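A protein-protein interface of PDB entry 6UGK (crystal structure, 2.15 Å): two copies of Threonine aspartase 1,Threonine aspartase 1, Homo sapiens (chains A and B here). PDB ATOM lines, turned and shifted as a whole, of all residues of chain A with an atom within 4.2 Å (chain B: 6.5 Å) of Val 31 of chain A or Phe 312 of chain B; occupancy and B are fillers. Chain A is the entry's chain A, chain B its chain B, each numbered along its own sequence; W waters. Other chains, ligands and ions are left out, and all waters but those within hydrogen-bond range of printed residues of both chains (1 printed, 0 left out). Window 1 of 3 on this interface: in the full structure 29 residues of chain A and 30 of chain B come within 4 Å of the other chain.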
ATOM      1  N   GLY A  29     -11.666 -21.746  22.818  1.00  0.00           N
ATOM      2  CA  GLY A  29     -10.483 -22.193  22.123  1.00  0.00           C
ATOM      3  C   GLY A  29      -9.805 -23.416  22.707  1.00  0.00           C
ATOM      4  O   GLY A  29      -8.810 -23.877  22.134  1.00  0.00           O
ATOM      5  N   ARG A  30     -10.297 -23.959  23.820  1.00  0.00           N
ATOM      6  CA  ARG A  30      -9.738 -25.198  24.349  1.00  0.00           C
ATOM      7  C   ARG A  30     -10.076 -26.341  23.410  1.00  0.00           C
ATOM      8  O   ARG A  30     -11.250 -26.626  23.170  1.00  0.00           O
ATOM      9  CB  ARG A  30     -10.274 -25.505  25.749  1.00  0.00           C
ATOM     10  CG  ARG A  30      -9.657 -26.783  26.350  1.00  0.00           C
ATOM     11  CD  ARG A  30     -10.219 -27.115  27.738  1.00  0.00           C
ATOM     12  NE  ARG A  30      -9.576 -28.287  28.346  1.00  0.00           N
ATOM     13  CZ  ARG A  30      -9.327 -28.405  29.649  1.00  0.00           C
ATOM     14  NH1 ARG A  30      -9.646 -27.419  30.488  1.00  0.00           N
ATOM     15  NH2 ARG A  30      -8.746 -29.503  30.121  1.00  0.00           N
ATOM     16  N   VAL A  31      -9.052 -27.020  22.917  1.00  0.00           N
ATOM     17  CA  VAL A  31      -9.215 -28.139  22.001  1.00  0.00           C
ATOM     18  C   VAL A  31      -8.797 -29.416  22.711  1.00  0.00           C
ATOM     19  O   VAL A  31      -7.791 -29.438  23.426  1.00  0.00           O
ATOM     20  CB  VAL A  31      -8.386 -27.909  20.725  1.00  0.00           C
ATOM     21  CG1 VAL A  31      -8.412 -29.145  19.845  1.00  0.00           C
ATOM     22  CG2 VAL A  31      -8.918 -26.665  19.989  1.00  0.00           C
ATOM     23  N   GLY A  32      -9.568 -30.482  22.521  1.00  0.00           N
ATOM     24  CA  GLY A  32      -9.270 -31.694  23.257  1.00  0.00           C
ATOM     25  C   GLY A  32      -9.021 -32.901  22.383  1.00  0.00           C
ATOM     26  O   GLY A  32      -8.761 -32.768  21.184  1.00  0.00           O
ATOM     27  N   ALA A  35      -9.985 -33.902  18.554  1.00  0.00           N
ATOM     28  CA  ALA A  35      -9.332 -33.244  17.437  1.00  0.00           C
ATOM     29  C   ALA A  35      -7.897 -33.699  17.210  1.00  0.00           C
ATOM     30  O   ALA A  35      -7.303 -33.311  16.198  1.00  0.00           O
ATOM     31  CB  ALA A  35      -9.325 -31.730  17.655  1.00  0.00           C
ATOM     32  N   LEU A  36      -7.313 -34.475  18.121  1.00  0.00           N
ATOM     33  CA  LEU A  36      -5.861 -34.619  18.152  1.00  0.00           C
ATOM     34  C   LEU A  36      -5.436 -35.951  17.572  1.00  0.00           C
ATOM     35  O   LEU A  36      -5.901 -37.015  18.012  1.00  0.00           O
ATOM     36  CB  LEU A  36      -5.327 -34.448  19.572  1.00  0.00           C
ATOM     37  CG  LEU A  36      -5.509 -33.013  20.076  1.00  0.00           C
ATOM     38  CD1 LEU A  36      -5.061 -32.885  21.521  1.00  0.00           C
ATOM     39  CD2 LEU A  36      -4.751 -32.030  19.201  1.00  0.00           C
ATOM     40  N   ASP A 264     -14.929 -30.329  18.462  1.00  0.00           N
ATOM     41  CA  ASP A 264     -13.733 -31.058  18.038  1.00  0.00           C
ATOM     42  C   ASP A 264     -14.163 -32.347  17.346  1.00  0.00           C
ATOM     43  O   ASP A 264     -15.127 -32.986  17.773  1.00  0.00           O
ATOM     44  CB  ASP A 264     -12.839 -31.426  19.236  1.00  0.00           C
ATOM     45  CG  ASP A 264     -12.449 -30.229  20.076  1.00  0.00           C
ATOM     46  OD1 ASP A 264     -12.364 -29.114  19.506  1.00  0.00           O
ATOM     47  OD2 ASP A 264     -12.222 -30.409  21.309  1.00  0.00           O
ATOM     48  N   ALA A 280     -12.270 -26.553  17.822  1.00  0.00           N
ATOM     49  CA  ALA A 280     -12.867 -25.273  18.207  1.00  0.00           C
ATOM     50  C   ALA A 280     -13.768 -24.729  17.099  1.00  0.00           C
ATOM     51  O   ALA A 280     -13.746 -23.537  16.778  1.00  0.00           O
ATOM     52  CB  ALA A 280     -11.781 -24.247  18.585  1.00  0.00           C
ATOM     53  N   VAL B  31      -3.401 -25.659  11.520  1.00  0.00           N
ATOM     54  CA  VAL B  31      -2.523 -25.910  12.653  1.00  0.00           C
ATOM     55  C   VAL B  31      -1.608 -27.069  12.281  1.00  0.00           C
ATOM     56  O   VAL B  31      -2.081 -28.111  11.816  1.00  0.00           O
ATOM     57  CB  VAL B  31      -3.335 -26.219  13.922  1.00  0.00           C
ATOM     58  CG1 VAL B  31      -2.401 -26.599  15.060  1.00  0.00           C
ATOM     59  CG2 VAL B  31      -4.180 -25.014  14.297  1.00  0.00           C
ATOM     60  N   ALA B  35       2.215 -27.528  17.284  1.00  0.00           N
ATOM     61  CA  ALA B  35       1.179 -27.419  18.302  1.00  0.00           C
ATOM     62  C   ALA B  35       0.709 -28.760  18.846  1.00  0.00           C
ATOM     63  O   ALA B  35      -0.009 -28.775  19.849  1.00  0.00           O
ATOM     64  CB  ALA B  35      -0.057 -26.680  17.741  1.00  0.00           C
ATOM     65  N   LEU B  36       1.052 -29.876  18.204  1.00  0.00           N
ATOM     66  CA  LEU B  36       0.402 -31.145  18.491  1.00  0.00           C
ATOM     67  C   LEU B  36       1.245 -31.960  19.456  1.00  0.00           C
ATOM     68  O   LEU B  36       2.443 -32.170  19.223  1.00  0.00           O
ATOM     69  CB  LEU B  36       0.154 -31.943  17.213  1.00  0.00           C
ATOM     70  CG  LEU B  36      -0.626 -31.170  16.141  1.00  0.00           C
ATOM     71  CD1 LEU B  36      -0.924 -32.067  14.942  1.00  0.00           C
ATOM     72  CD2 LEU B  36      -1.903 -30.602  16.721  1.00  0.00           C
ATOM     73  N   ALA B 265       2.874 -23.342  18.774  1.00  0.00           N
ATOM     74  CA  ALA B 265       3.994 -23.583  19.681  1.00  0.00           C
ATOM     75  C   ALA B 265       3.582 -24.594  20.742  1.00  0.00           C
ATOM     76  O   ALA B 265       2.401 -24.707  21.090  1.00  0.00           O
ATOM     77  CB  ALA B 265       4.479 -22.290  20.360  1.00  0.00           C
ATOM     78  N   PHE B 275       2.444 -30.400  29.792  1.00  0.00           N
ATOM     79  CA  PHE B 275       2.469 -29.977  28.400  1.00  0.00           C
ATOM     80  C   PHE B 275       1.651 -28.700  28.263  1.00  0.00           C
ATOM     81  O   PHE B 275       0.649 -28.524  28.965  1.00  0.00           O
ATOM     82  CB  PHE B 275       1.890 -31.087  27.517  1.00  0.00           C
ATOM     83  CG  PHE B 275       1.808 -30.745  26.054  1.00  0.00           C
ATOM     84  CD1 PHE B 275       2.936 -30.827  25.244  1.00  0.00           C
ATOM     85  CD2 PHE B 275       0.592 -30.401  25.475  1.00  0.00           C
ATOM     86  CE1 PHE B 275       2.856 -30.541  23.886  1.00  0.00           C
ATOM     87  CE2 PHE B 275       0.503 -30.115  24.116  1.00  0.00           C
ATOM     88  CZ  PHE B 275       1.636 -30.183  23.325  1.00  0.00           C
ATOM     89  N   GLY B 276       2.079 -27.810  27.383  1.00  0.00           N
ATOM     90  CA  GLY B 276       1.274 -26.645  27.033  1.00  0.00           C
ATOM     91  C   GLY B 276       1.412 -26.362  25.553  1.00  0.00           C
ATOM     92  O   GLY B 276       2.453 -26.638  24.948  1.00  0.00           O
ATOM     93  N   ALA B 277       0.349 -25.816  24.959  1.00  0.00           N
ATOM     94  CA  ALA B 277       0.415 -25.618  23.518  1.00  0.00           C
ATOM     95  C   ALA B 277      -0.586 -24.569  23.057  1.00  0.00           C
ATOM     96  O   ALA B 277      -1.661 -24.412  23.642  1.00  0.00           O
ATOM     97  CB  ALA B 277       0.190 -26.947  22.780  1.00  0.00           C
ATOM     98  N   VAL B 278      -0.219 -23.867  21.975  1.00  0.00           N
ATOM     99  CA  VAL B 278      -1.114 -22.973  21.257  1.00  0.00           C
ATOM    100  C   VAL B 278      -1.058 -23.264  19.761  1.00  0.00           C
ATOM    101  O   VAL B 278      -0.006 -23.614  19.212  1.00  0.00           O
ATOM    102  CB  VAL B 278      -0.770 -21.496  21.530  1.00  0.00           C
ATOM    103  CG1 VAL B 278      -1.020 -21.177  22.987  1.00  0.00           C
ATOM    104  CG2 VAL B 278       0.674 -21.198  21.124  1.00  0.00           C
ATOM    105  N   GLY B 279      -2.202 -23.118  19.100  1.00  0.00           N
ATOM    106  CA  GLY B 279      -2.265 -23.200  17.649  1.00  0.00           C
ATOM    107  C   GLY B 279      -3.036 -22.042  17.066  1.00  0.00           C
ATOM    108  O   GLY B 279      -3.976 -21.524  17.667  1.00  0.00           O
ATOM    109  N   ALA B 280      -2.633 -21.628  15.854  1.00  0.00           N
ATOM    110  CA  ALA B 280      -3.307 -20.555  15.132  1.00  0.00           C
ATOM    111  C   ALA B 280      -3.447 -19.305  15.997  1.00  0.00           C
ATOM    112  O   ALA B 280      -4.495 -18.660  16.036  1.00  0.00           O
ATOM    113  CB  ALA B 280      -4.669 -21.017  14.606  1.00  0.00           C
ATOM    114  N   LEU B 294       0.605 -21.921  29.966  1.00  0.00           N
ATOM    115  CA  LEU B 294      -0.394 -22.986  30.092  1.00  0.00           C
ATOM    116  C   LEU B 294       0.163 -24.166  30.882  1.00  0.00           C
ATOM    117  O   LEU B 294      -0.537 -24.760  31.715  1.00  0.00           O
ATOM    118  CB  LEU B 294      -0.865 -23.448  28.713  1.00  0.00           C
ATOM    119  CG  LEU B 294      -1.857 -22.539  27.971  1.00  0.00           C
ATOM    120  CD1 LEU B 294      -1.787 -22.801  26.478  1.00  0.00           C
ATOM    121  CD2 LEU B 294      -3.299 -22.737  28.481  1.00  0.00           C
ATOM    122  N   PRO B 309      -6.598 -27.985  34.207  1.00  0.00           N
ATOM    123  CA  PRO B 309      -6.559 -26.764  33.396  1.00  0.00           C
ATOM    124  C   PRO B 309      -6.320 -27.098  31.935  1.00  0.00           C
ATOM    125  O   PRO B 309      -5.852 -28.198  31.609  1.00  0.00           O
ATOM    126  CB  PRO B 309      -5.380 -25.980  33.995  1.00  0.00           C
ATOM    127  CG  PRO B 309      -5.217 -26.538  35.376  1.00  0.00           C
ATOM    128  CD  PRO B 309      -5.585 -27.985  35.274  1.00  0.00           C
ATOM    129  N   PRO B 310      -6.660 -26.192  31.021  1.00  0.00           N
ATOM    130  CA  PRO B 310      -6.410 -26.457  29.601  1.00  0.00           C
ATOM    131  C   PRO B 310      -4.918 -26.545  29.316  1.00  0.00           C
ATOM    132  O   PRO B 310      -4.124 -25.762  29.840  1.00  0.00           O
ATOM    133  CB  PRO B 310      -7.036 -25.242  28.905  1.00  0.00           C
ATOM    134  CG  PRO B 310      -6.892 -24.144  29.930  1.00  0.00           C
ATOM    135  CD  PRO B 310      -7.201 -24.839  31.240  1.00  0.00           C
ATOM    136  N   CYS B 311      -4.535 -27.501  28.469  1.00  0.00           N
ATOM    137  CA  CYS B 311      -3.167 -27.549  27.977  1.00  0.00           C
ATOM    138  C   CYS B 311      -3.026 -27.076  26.528  1.00  0.00           C
ATOM    139  O   CYS B 311      -1.909 -26.800  26.100  1.00  0.00           O
ATOM    140  CB  CYS B 311      -2.590 -28.968  28.133  1.00  0.00           C
ATOM    141  SG  CYS B 311      -3.274 -30.232  27.020  1.00  0.00           S
ATOM    142  N   PHE B 312      -4.118 -26.945  25.772  1.00  0.00           N
ATOM    143  CA  PHE B 312      -4.048 -26.635  24.338  1.00  0.00           C
ATOM    144  C   PHE B 312      -5.152 -25.640  23.997  1.00  0.00           C
ATOM    145  O   PHE B 312      -6.334 -25.995  24.050  1.00  0.00           O
ATOM    146  CB  PHE B 312      -4.188 -27.917  23.500  1.00  0.00           C
ATOM    147  CG  PHE B 312      -4.067 -27.702  21.989  1.00  0.00           C
ATOM    148  CD1 PHE B 312      -3.270 -26.691  21.461  1.00  0.00           C
ATOM    149  CD2 PHE B 312      -4.734 -28.550  21.110  1.00  0.00           C
ATOM    150  CE1 PHE B 312      -3.147 -26.515  20.071  1.00  0.00           C
ATOM    151  CE2 PHE B 312      -4.634 -28.392  19.741  1.00  0.00           C
ATOM    152  CZ  PHE B 312      -3.837 -27.368  19.208  1.00  0.00           C
ATOM    153  N   LEU B 313      -4.784 -24.392  23.663  1.00  0.00           N
ATOM    154  CA  LEU B 313      -5.744 -23.381  23.222  1.00  0.00           C
ATOM    155  C   LEU B 313      -5.419 -22.927  21.805  1.00  0.00           C
ATOM    156  O   LEU B 313      -4.255 -22.865  21.408  1.00  0.00           O
ATOM    157  CB  LEU B 313      -5.753 -22.137  24.127  1.00  0.00           C
ATOM    158  CG  LEU B 313      -6.030 -22.347  25.617  1.00  0.00           C
ATOM    159  CD1 LEU B 313      -5.951 -21.019  26.323  1.00  0.00           C
ATOM    160  CD2 LEU B 313      -7.412 -22.959  25.838  1.00  0.00           C
ATOM    161  N   VAL B 314      -6.452 -22.559  21.051  1.00  0.00           N
ATOM    162  CA  VAL B 314      -6.248 -22.101  19.686  1.00  0.00           C
ATOM    163  C   VAL B 314      -6.964 -20.776  19.472  1.00  0.00           C
ATOM    164  O   VAL B 314      -7.868 -20.404  20.224  1.00  0.00           O
ATOM    165  CB  VAL B 314      -6.731 -23.131  18.651  1.00  0.00           C
ATOM    166  CG1 VAL B 314      -5.972 -24.425  18.816  1.00  0.00           C
ATOM    167  CG2 VAL B 314      -8.267 -23.338  18.781  1.00  0.00           C
HETATM  168  O   HOH W   1      -6.728 -28.620  26.337  1.00  0.00           O
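Printed residues of chain B within 4 Å of Val 31 of chain A: Phe 312 (3.1 Å) and Val 314 (3.6 Å).
Gly 32 of chain A touches none of the printed residues of chain B.
Printed residues of chain B within 4 Å of Leu 36 of chain A: Phe 312.
Of the printed residues of chain B, Ala 280 of chain A touches Val 314.
Ala 280 of chain B touches none of the printed residues of chain A.
Of chain A, only Gly 29 (3.8 Å), Arg 30 (3.5 Å), Val 31 (3.1 Å) and Leu 36 (3.7 Å) come within 4 Å of Phe 312 of chain B.
Of the printed residues of chain A, Leu 313 of chain B touches Gly 29 (3.3 Å) and Arg 30 (3.6 Å).
Printed residues of chain A within 4 Å of Val 314 of chain B: Gly 29 (2.9 Å), Val 31 (3.6 Å) and Ala 280 (3.6 Å).
The nearest residue of chain B that does not touch Val 31 of chain A is Leu 313 of chain B (4.9 Å).
The nearest printed residue of chain A that does not touch Phe 312 of chain B is Gly 32 of chain A (5.4 Å).
Positions printed for both chains: 31, 35, 36 and 280.
Water W1 lies within hydrogen-bond range of N of Phe 312 of chain B (3.2 Å), O of Val 31 of chain A (3.2 Å) and N of Cys 311 of chain B (3.3 Å).
Hydrophobic or aromatic side chains of chain A within 4 Å of the printed part of chain B: Val 31, Leu 36 and Ala 280.
Along chain A the printed residues that touch a printed residue of chain B span positions 29 to 280.
Of the 17 printed residues of chain B, 5 touch a printed residue of chain A.
Among the printed residues, 11 pairs touch across the chains.
Among the printed residues, no Asp or Glu carboxylate lies within 4 Å of a Lys or Arg side-chain nitrogen of the other chain.
N of Val 314 of chain B is in hydrogen-bond range of O of Gly 29 of chain A, at 2.9 Å.
N of Val 31 of chain A is in hydrogen-bond range of O of Phe 312 of chain B (3.1 Å).
The guanidinium group (NH1) of Arg 30 of chain A sits close to the backbone nitrogen (N) of Pro 310 of chain B.
O of Gly 29 of chain A touches O of Phe 312 of chain B (3.8 Å).
CA of Leu 313 of chain B touches O of Gly 29 of chain A (3.3 Å).
NH2 of Arg 30 of chain A touches O of Pro 309 of chain B, 3.5 Å away.
Arg 30 of chain A touches Phe 312 of chain B (CA to O, 3.5 Å).
Leu 313 of chain B touches Arg 30 of chain A.
Val 31 of chain A touches Val 314 of chain B (CG2 to CG2, 3.6 Å).
Leu 36 of chain A touches Phe 312 of chain B (CD2 to CE2, 3.7 Å).
Ala 280 of chain A touches Val 314 of chain B.
The backbone NH (N) of Ala 280 of chain A is in hydrogen-bond range of the side-chain carboxylate (OD1) of Asp 264 of chain A (3.1 Å).
The backbone carbonyl oxygen (O) of Ala 277 of chain B is in hydrogen-bond range of the backbone NH (N) of Leu 313 of chain B, at 3.1 Å.
The backbone NH of Gly 279 of chain B is in hydrogen-bond range of the backbone carbonyl oxygen of Leu 313 of chain B (3.1 Å).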
